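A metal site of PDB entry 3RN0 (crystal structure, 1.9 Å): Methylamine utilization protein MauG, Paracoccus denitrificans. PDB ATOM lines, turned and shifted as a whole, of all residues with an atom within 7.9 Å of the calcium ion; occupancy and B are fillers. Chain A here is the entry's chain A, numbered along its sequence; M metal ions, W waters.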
ATOM      1  N   ARG A  39     -15.195  -6.720  -8.721  1.00  0.00           N
ATOM      2  CA  ARG A  39     -16.557  -6.191  -8.919  1.00  0.00           C
ATOM      3  C   ARG A  39     -17.385  -6.135  -7.673  1.00  0.00           C
ATOM      4  O   ARG A  39     -18.564  -6.337  -7.766  1.00  0.00           O
ATOM      5  CB  ARG A  39     -17.364  -6.959  -9.957  1.00  0.00           C
ATOM      6  CG  ARG A  39     -18.346  -6.008 -10.749  1.00  0.00           C
ATOM      7  CD  ARG A  39     -18.913  -6.751 -11.870  1.00  0.00           C
ATOM      8  NE  ARG A  39     -19.961  -6.075 -12.614  1.00  0.00           N
ATOM      9  CZ  ARG A  39     -21.249  -5.976 -12.306  1.00  0.00           C
ATOM     10  NH1 ARG A  39     -22.036  -5.309 -13.162  1.00  0.00           N
ATOM     11  NH2 ARG A  39     -21.729  -6.449 -11.148  1.00  0.00           N
ATOM     12  N   THR A  42     -19.144  -9.371  -6.896  1.00  0.00           N
ATOM     13  CA  THR A  42     -20.249  -9.850  -7.711  1.00  0.00           C
ATOM     14  C   THR A  42     -19.676 -10.400  -9.035  1.00  0.00           C
ATOM     15  O   THR A  42     -18.420 -10.441  -9.241  1.00  0.00           O
ATOM     16  CB  THR A  42     -21.314  -8.712  -7.951  1.00  0.00           C
ATOM     17  OG1 THR A  42     -20.751  -7.691  -8.744  1.00  0.00           O
ATOM     18  CG2 THR A  42     -21.774  -8.059  -6.689  1.00  0.00           C
ATOM     19  N   ASP A  43     -20.596 -10.811  -9.918  1.00  0.00           N
ATOM     20  CA  ASP A  43     -20.258 -11.585 -11.105  1.00  0.00           C
ATOM     21  C   ASP A  43     -20.240 -10.723 -12.355  1.00  0.00           C
ATOM     22  O   ASP A  43     -21.298 -10.301 -12.839  1.00  0.00           O
ATOM     23  CB  ASP A  43     -21.181 -12.781 -11.257  1.00  0.00           C
ATOM     24  CG  ASP A  43     -20.698 -13.776 -12.309  1.00  0.00           C
ATOM     25  OD1 ASP A  43     -21.313 -14.894 -12.468  1.00  0.00           O
ATOM     26  OD2 ASP A  43     -19.725 -13.440 -13.020  1.00  0.00           O
ATOM     27  N   LEU A  51     -25.984 -10.243 -17.338  1.00  0.00           N
ATOM     28  CA  LEU A  51     -25.409 -10.255 -15.999  1.00  0.00           C
ATOM     29  C   LEU A  51     -26.445 -10.542 -14.894  1.00  0.00           C
ATOM     30  O   LEU A  51     -26.143 -10.409 -13.686  1.00  0.00           O
ATOM     31  CB  LEU A  51     -24.730  -8.930 -15.714  1.00  0.00           C
ATOM     32  CG  LEU A  51     -23.229  -8.710 -15.677  1.00  0.00           C
ATOM     33  CD1 LEU A  51     -22.504  -9.495 -16.764  1.00  0.00           C
ATOM     34  CD2 LEU A  51     -22.970  -7.211 -15.893  1.00  0.00           C
ATOM     35  N   ALA A  52     -27.671 -10.896 -15.303  1.00  0.00           N
ATOM     36  CA  ALA A  52     -28.768 -11.037 -14.337  1.00  0.00           C
ATOM     37  C   ALA A  52     -28.497 -12.178 -13.404  1.00  0.00           C
ATOM     38  O   ALA A  52     -28.832 -12.073 -12.225  1.00  0.00           O
ATOM     39  CB  ALA A  52     -30.094 -11.239 -15.001  1.00  0.00           C
ATOM     40  N   ASN A  66     -29.753 -13.057  -8.963  1.00  0.00           N
ATOM     41  CA  ASN A  66     -28.579 -12.272  -9.151  1.00  0.00           C
ATOM     42  C   ASN A  66     -27.672 -12.540  -7.945  1.00  0.00           C
ATOM     43  O   ASN A  66     -28.098 -12.552  -6.742  1.00  0.00           O
ATOM     44  CB  ASN A  66     -29.012 -10.808  -9.194  1.00  0.00           C
ATOM     45  CG  ASN A  66     -27.900  -9.877  -9.595  1.00  0.00           C
ATOM     46  OD1 ASN A  66     -27.563  -8.957  -8.841  1.00  0.00           O
ATOM     47  ND2 ASN A  66     -27.305 -10.099 -10.774  1.00  0.00           N
ATOM     48  N   THR A  67     -26.404 -12.747  -8.268  1.00  0.00           N
ATOM     49  CA  THR A  67     -25.340 -12.874  -7.298  1.00  0.00           C
ATOM     50  C   THR A  67     -25.092 -11.529  -6.581  1.00  0.00           C
ATOM     51  O   THR A  67     -24.727 -10.547  -7.205  1.00  0.00           O
ATOM     52  CB  THR A  67     -24.087 -13.352  -8.019  1.00  0.00           C
ATOM     53  OG1 THR A  67     -24.346 -14.643  -8.630  1.00  0.00           O
ATOM     54  CG2 THR A  67     -22.877 -13.365  -7.012  1.00  0.00           C
ATOM     55  N   PRO A  68     -25.377 -11.455  -5.264  1.00  0.00           N
ATOM     56  CA  PRO A  68     -25.223 -10.228  -4.538  1.00  0.00           C
ATOM     57  C   PRO A  68     -23.782 -10.055  -4.084  1.00  0.00           C
ATOM     58  O   PRO A  68     -22.978 -11.016  -4.024  1.00  0.00           O
ATOM     59  CB  PRO A  68     -26.148 -10.411  -3.350  1.00  0.00           C
ATOM     60  CG  PRO A  68     -25.954 -11.829  -2.970  1.00  0.00           C
ATOM     61  CD  PRO A  68     -25.749 -12.556  -4.366  1.00  0.00           C
ATOM     62  N   THR A  69     -23.431  -8.822  -3.793  1.00  0.00           N
ATOM     63  CA  THR A  69     -22.181  -8.515  -3.116  1.00  0.00           C
ATOM     64  C   THR A  69     -21.975  -9.228  -1.776  1.00  0.00           C
ATOM     65  O   THR A  69     -22.926  -9.487  -0.996  1.00  0.00           O
ATOM     66  CB  THR A  69     -22.020  -6.991  -2.914  1.00  0.00           C
ATOM     67  OG1 THR A  69     -20.685  -6.727  -2.439  1.00  0.00           O
ATOM     68  CG2 THR A  69     -23.049  -6.458  -1.883  1.00  0.00           C
ATOM     69  N   TRP A  93     -31.080 -13.880  -0.655  1.00  0.00           N
ATOM     70  CA  TRP A  93     -32.122 -12.896  -0.892  1.00  0.00           C
ATOM     71  C   TRP A  93     -33.358 -13.354  -0.178  1.00  0.00           C
ATOM     72  O   TRP A  93     -34.278 -12.569   0.021  1.00  0.00           O
ATOM     73  CB  TRP A  93     -32.407 -12.817  -2.372  1.00  0.00           C
ATOM     74  CG  TRP A  93     -31.422 -12.087  -3.190  1.00  0.00           C
ATOM     75  CD1 TRP A  93     -30.441 -12.628  -3.970  1.00  0.00           C
ATOM     76  CD2 TRP A  93     -31.426 -10.660  -3.444  1.00  0.00           C
ATOM     77  NE1 TRP A  93     -29.788 -11.598  -4.675  1.00  0.00           N
ATOM     78  CE2 TRP A  93     -30.356 -10.389  -4.345  1.00  0.00           C
ATOM     79  CE3 TRP A  93     -32.195  -9.589  -2.949  1.00  0.00           C
ATOM     80  CZ2 TRP A  93     -30.056  -9.092  -4.804  1.00  0.00           C
ATOM     81  CZ3 TRP A  93     -31.884  -8.273  -3.405  1.00  0.00           C
ATOM     82  CH2 TRP A  93     -30.838  -8.052  -4.332  1.00  0.00           C
ATOM     83  N   ASN A 271     -22.064   0.170  -2.289  1.00  0.00           N
ATOM     84  CA  ASN A 271     -21.615  -0.309  -3.623  1.00  0.00           C
ATOM     85  C   ASN A 271     -22.731  -0.540  -4.655  1.00  0.00           C
ATOM     86  O   ASN A 271     -22.462  -0.960  -5.776  1.00  0.00           O
ATOM     87  CB  ASN A 271     -20.686  -1.536  -3.534  1.00  0.00           C
ATOM     88  CG  ASN A 271     -19.393  -1.249  -2.726  1.00  0.00           C
ATOM     89  OD1 ASN A 271     -18.716  -0.212  -2.920  1.00  0.00           O
ATOM     90  ND2 ASN A 271     -19.054  -2.182  -1.799  1.00  0.00           N
ATOM     91  N   VAL A 272     -23.951  -0.161  -4.331  1.00  0.00           N
ATOM     92  CA  VAL A 272     -25.058  -0.352  -5.311  1.00  0.00           C
ATOM     93  C   VAL A 272     -24.628   0.050  -6.735  1.00  0.00           C
ATOM     94  O   VAL A 272     -25.007  -0.604  -7.752  1.00  0.00           O
ATOM     95  CB  VAL A 272     -26.373   0.348  -4.802  1.00  0.00           C
ATOM     96  CG1 VAL A 272     -26.233   1.862  -4.697  1.00  0.00           C
ATOM     97  CG2 VAL A 272     -27.571  -0.039  -5.591  1.00  0.00           C
ATOM     98  N   VAL A 274     -22.006  -0.051  -8.373  1.00  0.00           N
ATOM     99  CA  VAL A 274     -21.043  -0.782  -9.196  1.00  0.00           C
ATOM    100  C   VAL A 274     -21.504  -2.243  -9.297  1.00  0.00           C
ATOM    101  O   VAL A 274     -20.858  -3.048  -9.966  1.00  0.00           O
ATOM    102  CB  VAL A 274     -19.551  -0.668  -8.719  1.00  0.00           C
ATOM    103  CG1 VAL A 274     -19.085   0.718  -8.909  1.00  0.00           C
ATOM    104  CG2 VAL A 274     -19.402  -1.169  -7.205  1.00  0.00           C
ATOM    105  N   THR A 275     -22.652  -2.545  -8.703  1.00  0.00           N
ATOM    106  CA  THR A 275     -23.121  -3.960  -8.654  1.00  0.00           C
ATOM    107  C   THR A 275     -24.406  -4.274  -9.454  1.00  0.00           C
ATOM    108  O   THR A 275     -25.145  -5.199  -9.105  1.00  0.00           O
ATOM    109  CB  THR A 275     -23.278  -4.422  -7.203  1.00  0.00           C
ATOM    110  OG1 THR A 275     -24.312  -3.629  -6.625  1.00  0.00           O
ATOM    111  CG2 THR A 275     -21.984  -4.198  -6.448  1.00  0.00           C
ATOM    112  N   GLY A 276     -24.660  -3.514 -10.520  1.00  0.00           N
ATOM    113  CA  GLY A 276     -25.785  -3.837 -11.396  1.00  0.00           C
ATOM    114  C   GLY A 276     -25.638  -5.231 -12.047  1.00  0.00           C
ATOM    115  O   GLY A 276     -24.536  -5.791 -12.104  1.00  0.00           O
ATOM    116  N   PRO A 277     -26.723  -5.781 -12.598  1.00  0.00           N
ATOM    117  CA  PRO A 277     -28.045  -5.251 -12.615  1.00  0.00           C
ATOM    118  C   PRO A 277     -28.631  -5.472 -11.234  1.00  0.00           C
ATOM    119  O   PRO A 277     -27.986  -6.036 -10.321  1.00  0.00           O
ATOM    120  CB  PRO A 277     -28.764  -6.097 -13.694  1.00  0.00           C
ATOM    121  CG  PRO A 277     -27.971  -7.335 -13.829  1.00  0.00           C
ATOM    122  CD  PRO A 277     -26.685  -7.177 -13.094  1.00  0.00           C
ATOM    123  N   TYR A 278     -29.877  -5.069 -11.095  1.00  0.00           N
ATOM    124  CA  TYR A 278     -30.435  -4.786  -9.769  1.00  0.00           C
ATOM    125  C   TYR A 278     -31.622  -5.656  -9.555  1.00  0.00           C
ATOM    126  O   TYR A 278     -32.193  -6.252 -10.509  1.00  0.00           O
ATOM    127  CB  TYR A 278     -30.820  -3.326  -9.707  1.00  0.00           C
ATOM    128  CG  TYR A 278     -29.598  -2.484  -9.809  1.00  0.00           C
ATOM    129  CD1 TYR A 278     -29.256  -1.854 -11.033  1.00  0.00           C
ATOM    130  CD2 TYR A 278     -28.696  -2.438  -8.742  1.00  0.00           C
ATOM    131  CE1 TYR A 278     -28.097  -1.156 -11.122  1.00  0.00           C
ATOM    132  CE2 TYR A 278     -27.551  -1.715  -8.795  1.00  0.00           C
ATOM    133  CZ  TYR A 278     -27.250  -1.080  -9.988  1.00  0.00           C
ATOM    134  OH  TYR A 278     -26.079  -0.359 -10.097  1.00  0.00           O
ATOM    135  N   MET A 279     -31.927  -5.743  -8.262  1.00  0.00           N
ATOM    136  CA  MET A 279     -32.959  -6.566  -7.686  1.00  0.00           C
ATOM    137  C   MET A 279     -32.537  -8.026  -7.655  1.00  0.00           C
ATOM    138  O   MET A 279     -31.550  -8.439  -8.290  1.00  0.00           O
ATOM    139  CB  MET A 279     -34.343  -6.338  -8.365  1.00  0.00           C
ATOM    140  CG  MET A 279     -34.805  -4.872  -8.366  1.00  0.00           C
ATOM    141  SD  MET A 279     -34.814  -4.121  -6.724  1.00  0.00           S
ATOM    142  CE  MET A 279     -35.096  -2.376  -7.132  1.00  0.00           C
ATOM    143  N   HIS A 280     -33.304  -8.785  -6.924  1.00  0.00           N
ATOM    144  CA  HIS A 280     -33.027 -10.171  -6.673  1.00  0.00           C
ATOM    145  C   HIS A 280     -32.839 -10.953  -7.952  1.00  0.00           C
ATOM    146  O   HIS A 280     -32.155 -11.927  -7.930  1.00  0.00           O
ATOM    147  CB  HIS A 280     -34.107 -10.759  -5.726  1.00  0.00           C
ATOM    148  CG  HIS A 280     -35.436 -10.985  -6.394  1.00  0.00           C
ATOM    149  ND1 HIS A 280     -36.511 -10.127  -6.270  1.00  0.00           N
ATOM    150  CD2 HIS A 280     -35.858 -11.988  -7.223  1.00  0.00           C
ATOM    151  CE1 HIS A 280     -37.527 -10.584  -6.975  1.00  0.00           C
ATOM    152  NE2 HIS A 280     -37.158 -11.705  -7.576  1.00  0.00           N
ATOM    153  N   ASN A 281     -33.389 -10.486  -9.086  1.00  0.00           N
ATOM    154  CA  ASN A 281     -33.381 -11.282 -10.332  1.00  0.00           C
ATOM    155  C   ASN A 281     -32.605 -10.552 -11.432  1.00  0.00           C
ATOM    156  O   ASN A 281     -32.655 -10.957 -12.609  1.00  0.00           O
ATOM    157  CB  ASN A 281     -34.815 -11.585 -10.832  1.00  0.00           C
ATOM    158  CG  ASN A 281     -35.652 -10.340 -10.935  1.00  0.00           C
ATOM    159  OD1 ASN A 281     -35.100  -9.255 -10.824  1.00  0.00           O
ATOM    160  ND2 ASN A 281     -36.982 -10.480 -11.023  1.00  0.00           N
ATOM    161  N   GLY A 282     -31.968  -9.455 -11.050  1.00  0.00           N
ATOM    162  CA  GLY A 282     -31.145  -8.632 -11.981  1.00  0.00           C
ATOM    163  C   GLY A 282     -31.989  -8.072 -13.091  1.00  0.00           C
ATOM    164  O   GLY A 282     -31.474  -7.900 -14.205  1.00  0.00           O
ATOM    165  N   VAL A 283     -33.268  -7.809 -12.844  1.00  0.00           N
ATOM    166  CA  VAL A 283     -34.119  -7.390 -13.975  1.00  0.00           C
ATOM    167  C   VAL A 283     -33.743  -6.028 -14.580  1.00  0.00           C
ATOM    168  O   VAL A 283     -33.951  -5.802 -15.763  1.00  0.00           O
ATOM    169  CB  VAL A 283     -35.618  -7.461 -13.670  1.00  0.00           C
ATOM    170  CG1 VAL A 283     -35.966  -6.731 -12.295  1.00  0.00           C
ATOM    171  CG2 VAL A 283     -36.382  -6.843 -14.796  1.00  0.00           C
ATOM    172  N   PHE A 284     -33.204  -5.116 -13.781  1.00  0.00           N
ATOM    173  CA  PHE A 284     -32.863  -3.805 -14.258  1.00  0.00           C
ATOM    174  C   PHE A 284     -31.378  -3.655 -14.356  1.00  0.00           C
ATOM    175  O   PHE A 284     -30.657  -3.810 -13.354  1.00  0.00           O
ATOM    176  CB  PHE A 284     -33.361  -2.718 -13.285  1.00  0.00           C
ATOM    177  CG  PHE A 284     -34.808  -2.824 -12.966  1.00  0.00           C
ATOM    178  CD1 PHE A 284     -35.739  -3.107 -13.975  1.00  0.00           C
ATOM    179  CD2 PHE A 284     -35.252  -2.638 -11.663  1.00  0.00           C
ATOM    180  CE1 PHE A 284     -37.043  -3.216 -13.709  1.00  0.00           C
ATOM    181  CE2 PHE A 284     -36.604  -2.737 -11.365  1.00  0.00           C
ATOM    182  CZ  PHE A 284     -37.495  -3.011 -12.383  1.00  0.00           C
HETATM  183 CA    CA M   1     -26.781  -6.911  -8.524  1.00  0.00          CA
HETATM  184  O   HOH W   1     -25.171  -7.626  -7.047  1.00  0.00           O
HETATM  185  O   HOH W   2     -25.178  -7.915 -10.184  1.00  0.00           O
HETATM  186  O   HOH W   3     -26.639  -5.021  -7.054  1.00  0.00           O
HETATM  187  O   HOH W   4     -28.809  -7.035  -7.289  1.00  0.00           O
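The calcium ion is bound by OD1 of Asn 66, water W1, O of Pro 277, water W4, water W3, O of Thr 275 and water W2.
The calcium ion has seven donor atoms within binding distance.
The backbone carbonyl oxygen of Asn 66 sits at hydrogen-bond distance from the indole nitrogen of Trp 93, at 2.8 Å.
The side-chain amide nitrogen (ND2) of Asn 66 is in hydrogen-bond range of the backbone carbonyl oxygen (O) of Leu 51 (3.2 Å).
The side-chain amide nitrogen of Asn 66 is in hydrogen-bond range of the backbone carbonyl oxygen of Ala 52 (2.9 Å).
N of Asn 66 is in hydrogen-bond range of O of His 280 (2.8 Å).
The side-chain hydroxyl of Thr 275 lies within hydrogen-bond range of the backbone carbonyl oxygen of Val 272 (3.3 Å).
The backbone carbonyl oxygen of Asn 271 sits close to the side-chain hydroxyl of Thr 275, 3.4 Å away.
Three residues have an atom within 4 Å of the calcium ion: Asn 66, Thr 275 and Pro 277.
Water W2 lies within hydrogen-bond range of the backbone carbonyl oxygen (O) of Gly 276 (2.9 Å) and the side-chain amide nitrogen (ND2) of Asn 66 (3.1 Å).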
